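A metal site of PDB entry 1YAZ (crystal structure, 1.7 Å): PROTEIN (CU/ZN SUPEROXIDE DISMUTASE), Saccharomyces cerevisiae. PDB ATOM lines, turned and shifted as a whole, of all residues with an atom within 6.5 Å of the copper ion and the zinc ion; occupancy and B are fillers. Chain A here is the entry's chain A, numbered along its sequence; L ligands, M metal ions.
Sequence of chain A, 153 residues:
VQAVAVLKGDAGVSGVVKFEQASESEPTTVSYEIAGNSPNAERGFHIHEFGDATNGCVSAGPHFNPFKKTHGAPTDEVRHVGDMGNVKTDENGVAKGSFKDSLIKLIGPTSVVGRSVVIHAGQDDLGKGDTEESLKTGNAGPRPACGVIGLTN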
ATOM      1  N   GLY A  44      18.759  13.879   8.200  1.00  0.00           N
ATOM      2  CA  GLY A  44      17.664  12.908   8.269  1.00  0.00           C
ATOM      3  C   GLY A  44      17.968  11.649   7.489  1.00  0.00           C
ATOM      4  O   GLY A  44      18.468  11.704   6.372  1.00  0.00           O
ATOM      5  N   PHE A  45      17.648  10.506   8.083  1.00  0.00           N
ATOM      6  CA  PHE A  45      18.037   9.206   7.424  1.00  0.00           C
ATOM      7  C   PHE A  45      16.823   8.288   7.571  1.00  0.00           C
ATOM      8  O   PHE A  45      16.450   7.940   8.704  1.00  0.00           O
ATOM      9  CB  PHE A  45      19.208   8.699   8.313  1.00  0.00           C
ATOM     10  CG  PHE A  45      19.850   7.424   7.832  1.00  0.00           C
ATOM     11  CD1 PHE A  45      20.147   7.216   6.503  1.00  0.00           C
ATOM     12  CD2 PHE A  45      20.098   6.410   8.762  1.00  0.00           C
ATOM     13  CE1 PHE A  45      20.747   6.042   6.086  1.00  0.00           C
ATOM     14  CE2 PHE A  45      20.784   5.271   8.358  1.00  0.00           C
ATOM     15  CZ  PHE A  45      21.085   5.080   7.028  1.00  0.00           C
ATOM     16  N   HIS A  46      16.147   8.001   6.459  1.00  0.00           N
ATOM     17  CA  HIS A  46      14.861   7.293   6.581  1.00  0.00           C
ATOM     18  C   HIS A  46      14.715   6.162   5.556  1.00  0.00           C
ATOM     19  O   HIS A  46      15.344   6.104   4.525  1.00  0.00           O
ATOM     20  CB  HIS A  46      13.747   8.327   6.207  1.00  0.00           C
ATOM     21  CG  HIS A  46      13.822   9.571   7.035  1.00  0.00           C
ATOM     22  ND1 HIS A  46      13.580  10.815   6.497  1.00  0.00           N
ATOM     23  CD2 HIS A  46      14.103   9.758   8.348  1.00  0.00           C
ATOM     24  CE1 HIS A  46      13.697  11.724   7.444  1.00  0.00           C
ATOM     25  NE2 HIS A  46      14.011  11.115   8.594  1.00  0.00           N
ATOM     26  N   ILE A  47      13.737   5.278   5.869  1.00  0.00           N
ATOM     27  CA  ILE A  47      13.370   4.245   4.890  1.00  0.00           C
ATOM     28  C   ILE A  47      12.000   4.663   4.339  1.00  0.00           C
ATOM     29  O   ILE A  47      11.103   5.003   5.105  1.00  0.00           O
ATOM     30  CB  ILE A  47      13.195   2.863   5.604  1.00  0.00           C
ATOM     31  CG1 ILE A  47      14.590   2.406   6.086  1.00  0.00           C
ATOM     32  CG2 ILE A  47      12.665   1.877   4.510  1.00  0.00           C
ATOM     33  CD1 ILE A  47      14.711   1.091   6.704  1.00  0.00           C
ATOM     34  N   HIS A  48      11.976   4.805   3.027  1.00  0.00           N
ATOM     35  CA  HIS A  48      10.797   5.274   2.305  1.00  0.00           C
ATOM     36  C   HIS A  48      10.058   4.102   1.688  1.00  0.00           C
ATOM     37  O   HIS A  48      10.636   3.017   1.540  1.00  0.00           O
ATOM     38  CB  HIS A  48      11.198   6.281   1.239  1.00  0.00           C
ATOM     39  CG  HIS A  48      11.604   7.607   1.842  1.00  0.00           C
ATOM     40  ND1 HIS A  48      11.161   8.783   1.312  1.00  0.00           N
ATOM     41  CD2 HIS A  48      12.425   7.899   2.856  1.00  0.00           C
ATOM     42  CE1 HIS A  48      11.707   9.793   2.008  1.00  0.00           C
ATOM     43  NE2 HIS A  48      12.461   9.310   2.956  1.00  0.00           N
ATOM     44  N   PRO A  62       6.828   8.450   0.276  1.00  0.00           N
ATOM     45  CA  PRO A  62       6.941   8.955   1.651  1.00  0.00           C
ATOM     46  C   PRO A  62       7.591   7.924   2.567  1.00  0.00           C
ATOM     47  O   PRO A  62       8.040   6.865   2.139  1.00  0.00           O
ATOM     48  CB  PRO A  62       5.419   9.051   2.050  1.00  0.00           C
ATOM     49  CG  PRO A  62       4.860   7.834   1.402  1.00  0.00           C
ATOM     50  CD  PRO A  62       5.544   7.765   0.038  1.00  0.00           C
ATOM     51  N   HIS A  63       7.659   8.240   3.858  1.00  0.00           N
ATOM     52  CA  HIS A  63       8.312   7.250   4.766  1.00  0.00           C
ATOM     53  C   HIS A  63       7.442   5.971   4.870  1.00  0.00           C
ATOM     54  O   HIS A  63       6.208   6.000   4.816  1.00  0.00           O
ATOM     55  CB  HIS A  63       8.349   7.897   6.174  1.00  0.00           C
ATOM     56  CG  HIS A  63       9.380   8.988   6.216  1.00  0.00           C
ATOM     57  ND1 HIS A  63       9.636   9.778   7.282  1.00  0.00           N
ATOM     58  CD2 HIS A  63      10.262   9.392   5.229  1.00  0.00           C
ATOM     59  CE1 HIS A  63      10.619  10.622   7.033  1.00  0.00           C
ATOM     60  NE2 HIS A  63      10.980  10.399   5.772  1.00  0.00           N
ATOM     61  N   PHE A  64       8.153   4.860   5.028  1.00  0.00           N
ATOM     62  CA  PHE A  64       7.506   3.554   5.201  1.00  0.00           C
ATOM     63  C   PHE A  64       6.727   3.570   6.524  1.00  0.00           C
ATOM     64  O   PHE A  64       7.312   3.808   7.567  1.00  0.00           O
ATOM     65  CB  PHE A  64       8.532   2.455   5.181  1.00  0.00           C
ATOM     66  CG  PHE A  64       7.895   1.046   5.231  1.00  0.00           C
ATOM     67  CD1 PHE A  64       6.783   0.754   4.498  1.00  0.00           C
ATOM     68  CD2 PHE A  64       8.439   0.106   6.085  1.00  0.00           C
ATOM     69  CE1 PHE A  64       6.186  -0.512   4.618  1.00  0.00           C
ATOM     70  CE2 PHE A  64       7.876  -1.175   6.171  1.00  0.00           C
ATOM     71  CZ  PHE A  64       6.739  -1.455   5.449  1.00  0.00           C
ATOM     72  N   THR A  70       2.371   8.984  13.080  1.00  0.00           N
ATOM     73  CA  THR A  70       3.010  10.222  12.586  1.00  0.00           C
ATOM     74  C   THR A  70       4.519  10.055  12.736  1.00  0.00           C
ATOM     75  O   THR A  70       5.043   9.208  13.450  1.00  0.00           O
ATOM     76  CB  THR A  70       2.538  11.431  13.418  1.00  0.00           C
ATOM     77  OG1 THR A  70       2.589  11.105  14.806  1.00  0.00           O
ATOM     78  CG2 THR A  70       1.085  11.778  13.091  1.00  0.00           C
ATOM     79  N   HIS A  71       5.240  10.961  12.095  1.00  0.00           N
ATOM     80  CA  HIS A  71       6.705  10.898  12.130  1.00  0.00           C
ATOM     81  C   HIS A  71       7.258  11.148  13.508  1.00  0.00           C
ATOM     82  O   HIS A  71       6.753  11.994  14.278  1.00  0.00           O
ATOM     83  CB  HIS A  71       7.183  12.067  11.192  1.00  0.00           C
ATOM     84  CG  HIS A  71       8.677  12.110  11.083  1.00  0.00           C
ATOM     85  ND1 HIS A  71       9.365  11.194  10.303  1.00  0.00           N
ATOM     86  CD2 HIS A  71       9.582  12.957  11.617  1.00  0.00           C
ATOM     87  CE1 HIS A  71      10.667  11.482  10.384  1.00  0.00           C
ATOM     88  NE2 HIS A  71      10.829  12.534  11.184  1.00  0.00           N
ATOM     89  N   GLY A  72       8.384  10.505  13.832  1.00  0.00           N
ATOM     90  CA  GLY A  72       9.017  10.733  15.110  1.00  0.00           C
ATOM     91  C   GLY A  72      10.469  10.319  15.158  1.00  0.00           C
ATOM     92  O   GLY A  72      11.090  10.020  14.124  1.00  0.00           O
ATOM     93  N   ARG A  79       6.087   6.635  15.892  1.00  0.00           N
ATOM     94  CA  ARG A  79       7.025   6.962  14.795  1.00  0.00           C
ATOM     95  C   ARG A  79       6.607   6.123  13.564  1.00  0.00           C
ATOM     96  O   ARG A  79       5.838   5.174  13.718  1.00  0.00           O
ATOM     97  CB  ARG A  79       8.457   6.510  15.184  1.00  0.00           C
ATOM     98  CG  ARG A  79       8.580   5.062  15.624  1.00  0.00           C
ATOM     99  CD  ARG A  79      10.047   4.659  15.841  1.00  0.00           C
ATOM    100  NE  ARG A  79      10.601   4.069  14.607  1.00  0.00           N
ATOM    101  CZ  ARG A  79      11.626   3.230  14.584  1.00  0.00           C
ATOM    102  NH1 ARG A  79      12.365   2.993  15.662  1.00  0.00           N
ATOM    103  NH2 ARG A  79      11.922   2.565  13.447  1.00  0.00           N
ATOM    104  N   HIS A  80       7.158   6.474  12.449  1.00  0.00           N
ATOM    105  CA  HIS A  80       6.997   5.626  11.223  1.00  0.00           C
ATOM    106  C   HIS A  80       7.961   4.449  11.409  1.00  0.00           C
ATOM    107  O   HIS A  80       9.037   4.612  12.006  1.00  0.00           O
ATOM    108  CB  HIS A  80       7.471   6.464  10.038  1.00  0.00           C
ATOM    109  CG  HIS A  80       6.537   7.605   9.754  1.00  0.00           C
ATOM    110  ND1 HIS A  80       6.938   8.786   9.210  1.00  0.00           N
ATOM    111  CD2 HIS A  80       5.202   7.709   9.925  1.00  0.00           C
ATOM    112  CE1 HIS A  80       5.905   9.592   8.989  1.00  0.00           C
ATOM    113  NE2 HIS A  80       4.817   8.952   9.442  1.00  0.00           N
ATOM    114  N   GLY A  82       9.829   3.564   9.140  1.00  0.00           N
ATOM    115  CA  GLY A  82      11.043   4.010   8.438  1.00  0.00           C
ATOM    116  C   GLY A  82      11.858   5.062   9.136  1.00  0.00           C
ATOM    117  O   GLY A  82      12.890   5.522   8.617  1.00  0.00           O
ATOM    118  N   ASP A  83      11.487   5.563  10.324  1.00  0.00           N
ATOM    119  CA  ASP A  83      12.215   6.727  10.865  1.00  0.00           C
ATOM    120  C   ASP A  83      13.493   6.330  11.568  1.00  0.00           C
ATOM    121  O   ASP A  83      13.427   5.833  12.706  1.00  0.00           O
ATOM    122  CB  ASP A  83      11.264   7.367  11.975  1.00  0.00           C
ATOM    123  CG  ASP A  83      10.133   8.117  11.270  1.00  0.00           C
ATOM    124  OD1 ASP A  83      10.262   8.354  10.052  1.00  0.00           O
ATOM    125  OD2 ASP A  83       9.133   8.497  11.925  1.00  0.00           O
ATOM    126  N   VAL A 118      16.868   6.708   2.143  1.00  0.00           N
ATOM    127  CA  VAL A 118      17.078   8.088   1.682  1.00  0.00           C
ATOM    128  C   VAL A 118      17.903   8.831   2.740  1.00  0.00           C
ATOM    129  O   VAL A 118      17.584   8.733   3.904  1.00  0.00           O
ATOM    130  CB  VAL A 118      15.712   8.804   1.543  1.00  0.00           C
ATOM    131  CG1 VAL A 118      15.940  10.310   1.407  1.00  0.00           C
ATOM    132  CG2 VAL A 118      15.020   8.276   0.264  1.00  0.00           C
ATOM    133  N   HIS A 120      18.831  12.685   3.762  1.00  0.00           N
ATOM    134  CA  HIS A 120      18.299  14.016   3.346  1.00  0.00           C
ATOM    135  C   HIS A 120      19.412  15.075   3.460  1.00  0.00           C
ATOM    136  O   HIS A 120      20.477  14.829   4.013  1.00  0.00           O
ATOM    137  CB  HIS A 120      17.196  14.391   4.393  1.00  0.00           C
ATOM    138  CG  HIS A 120      15.885  13.738   4.080  1.00  0.00           C
ATOM    139  ND1 HIS A 120      14.936  14.287   3.238  1.00  0.00           N
ATOM    140  CD2 HIS A 120      15.330  12.601   4.608  1.00  0.00           C
ATOM    141  CE1 HIS A 120      13.837  13.509   3.255  1.00  0.00           C
ATOM    142  NE2 HIS A 120      14.098  12.480   4.038  1.00  0.00           N
ATOM    143  N   ASP A 124      16.549  16.301  10.614  1.00  0.00           N
ATOM    144  CA  ASP A 124      15.116  15.791  10.867  1.00  0.00           C
ATOM    145  C   ASP A 124      14.706  16.403  12.219  1.00  0.00           C
ATOM    146  O   ASP A 124      15.496  16.279  13.179  1.00  0.00           O
ATOM    147  CB  ASP A 124      15.306  14.263  11.066  1.00  0.00           C
ATOM    148  CG  ASP A 124      13.986  13.543  11.272  1.00  0.00           C
ATOM    149  OD1 ASP A 124      13.048  14.164  11.806  1.00  0.00           O
ATOM    150  OD2 ASP A 124      13.890  12.335  10.951  1.00  0.00           O
ATOM    151  N   LEU A 135       5.231  16.476  11.132  1.00  0.00           N
ATOM    152  CA  LEU A 135       4.596  15.227  11.445  1.00  0.00           C
ATOM    153  C   LEU A 135       4.614  14.249  10.289  1.00  0.00           C
ATOM    154  O   LEU A 135       4.240  13.076  10.519  1.00  0.00           O
ATOM    155  CB  LEU A 135       3.181  15.414  11.975  1.00  0.00           C
ATOM    156  CG  LEU A 135       3.094  16.214  13.303  1.00  0.00           C
ATOM    157  CD1 LEU A 135       1.609  16.350  13.688  1.00  0.00           C
ATOM    158  CD2 LEU A 135       3.813  15.408  14.398  1.00  0.00           C
ATOM    159  N   LYS A 136       5.088  14.687   9.137  1.00  0.00           N
ATOM    160  CA  LYS A 136       5.217  13.855   7.967  1.00  0.00           C
ATOM    161  C   LYS A 136       6.639  13.459   7.653  1.00  0.00           C
ATOM    162  O   LYS A 136       6.972  12.303   7.384  1.00  0.00           O
ATOM    163  CB  LYS A 136       4.590  14.516   6.735  1.00  0.00           C
ATOM    164  CG  LYS A 136       3.103  14.868   6.953  1.00  0.00           C
ATOM    165  CD  LYS A 136       2.879  15.080   8.455  1.00  0.00           C
ATOM    166  CE  LYS A 136       1.478  15.657   8.705  1.00  0.00           C
ATOM    167  NZ  LYS A 136       0.796  14.951   9.840  1.00  0.00           N
ATOM    168  N   THR A 137       7.542  14.436   7.568  1.00  0.00           N
ATOM    169  CA  THR A 137       8.905  14.070   7.121  1.00  0.00           C
ATOM    170  C   THR A 137       9.951  14.525   8.115  1.00  0.00           C
ATOM    171  O   THR A 137      11.137  14.309   7.892  1.00  0.00           O
ATOM    172  CB  THR A 137       9.221  14.858   5.800  1.00  0.00           C
ATOM    173  OG1 THR A 137       9.212  16.270   6.202  1.00  0.00           O
ATOM    174  CG2 THR A 137       8.072  14.711   4.835  1.00  0.00           C
ATOM    175  N   GLY A 138       9.556  15.277   9.154  1.00  0.00           N
ATOM    176  CA  GLY A 138      10.564  15.813  10.068  1.00  0.00           C
ATOM    177  C   GLY A 138      11.163  17.109   9.488  1.00  0.00           C
ATOM    178  O   GLY A 138      12.166  17.575  10.030  1.00  0.00           O
ATOM    179  N   ALA A 140      12.901  17.408   6.905  1.00  0.00           N
ATOM    180  CA  ALA A 140      14.293  17.090   6.611  1.00  0.00           C
ATOM    181  C   ALA A 140      14.785  17.592   5.283  1.00  0.00           C
ATOM    182  O   ALA A 140      15.988  17.433   4.984  1.00  0.00           O
ATOM    183  CB  ALA A 140      14.566  15.613   6.780  1.00  0.00           C
ATOM    184  N   GLY A 141      13.937  18.190   4.443  1.00  0.00           N
ATOM    185  CA  GLY A 141      14.396  18.780   3.206  1.00  0.00           C
ATOM    186  C   GLY A 141      14.645  17.812   2.073  1.00  0.00           C
ATOM    187  O   GLY A 141      14.139  16.684   2.046  1.00  0.00           O
ATOM    188  N   ARG A 143      16.404  15.397  -0.979  1.00  0.00           N
ATOM    189  CA  ARG A 143      16.895  14.023  -0.886  1.00  0.00           C
ATOM    190  C   ARG A 143      18.069  13.889  -1.891  1.00  0.00           C
ATOM    191  O   ARG A 143      17.833  13.447  -3.008  1.00  0.00           O
ATOM    192  CB  ARG A 143      15.738  13.114  -1.496  1.00  0.00           C
ATOM    193  CG  ARG A 143      14.458  13.278  -0.703  1.00  0.00           C
ATOM    194  CD  ARG A 143      13.332  12.415  -1.334  1.00  0.00           C
ATOM    195  NE  ARG A 143      12.086  12.648  -0.554  1.00  0.00           N
ATOM    196  CZ  ARG A 143      10.997  11.917  -0.740  1.00  0.00           C
ATOM    197  NH1 ARG A 143      11.023  10.893  -1.596  1.00  0.00           N
ATOM    198  NH2 ARG A 143       9.898  12.179  -0.052  1.00  0.00           N
HETATM  199  N1  LIG L   1      11.107  12.448   3.637  1.00  0.00           N
HETATM  200  N2  LIG L   1       9.995  12.010   3.524  1.00  0.00           N
HETATM  201  N3  LIG L   1       8.955  11.643   3.009  1.00  0.00           N
HETATM  202 CU    CU M   1      12.509  11.344   4.822  1.00  0.00          CU
HETATM  203 ZN    ZN M   2       8.967   9.527   9.192  1.00  0.00          ZN
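The backbone NH (N) of Gly 72 sits at hydrogen-bond distance from the side-chain carboxylate (OD2) of Asp 83, 2.9 Å away.
NE2 of His 63 lies close to NE2 of His 48 (3.4 Å).
OD1 of Asp 124 lies within hydrogen-bond range of NE2 of His 71 (2.8 Å).
N of His 71 lies within hydrogen-bond range of O of Leu 135 (2.8 Å).
The backbone carbonyl oxygen (O) of His 46 lies within hydrogen-bond range of the backbone NH (N) of Val 118.
NE2 of His 46 sits at hydrogen-bond distance from OD2 of Asp 124 (2.7 Å).
O of Gly 44 sits at hydrogen-bond distance from N of His 120, 2.8 Å away.
O of Gly 141 lies within hydrogen-bond range of ND1 of His 120 (2.8 Å).
Lys 136 touches the zinc ion (O to ZN, 3.9 Å).
Of the 25 residues printed, 5 come within 4 Å of the zinc ion.
The copper ion is bound by NE2 of His 63 (2.0 Å), ND1 of His 46 (2.1 Å), NE2 of His 120 (2.1 Å) and N1 of the ligand (2.1 Å).
The copper ion has four donor atoms within binding distance.
Slightly farther from the copper ion lies a ring nitrogen (NE2) of His 48 (2.8 Å).
The zinc ion is bound by OD1 of Asp 83, ND1 of His 63, ND1 of His 71 and ND1 of His 80.
The zinc ion has four donor atoms within binding distance.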
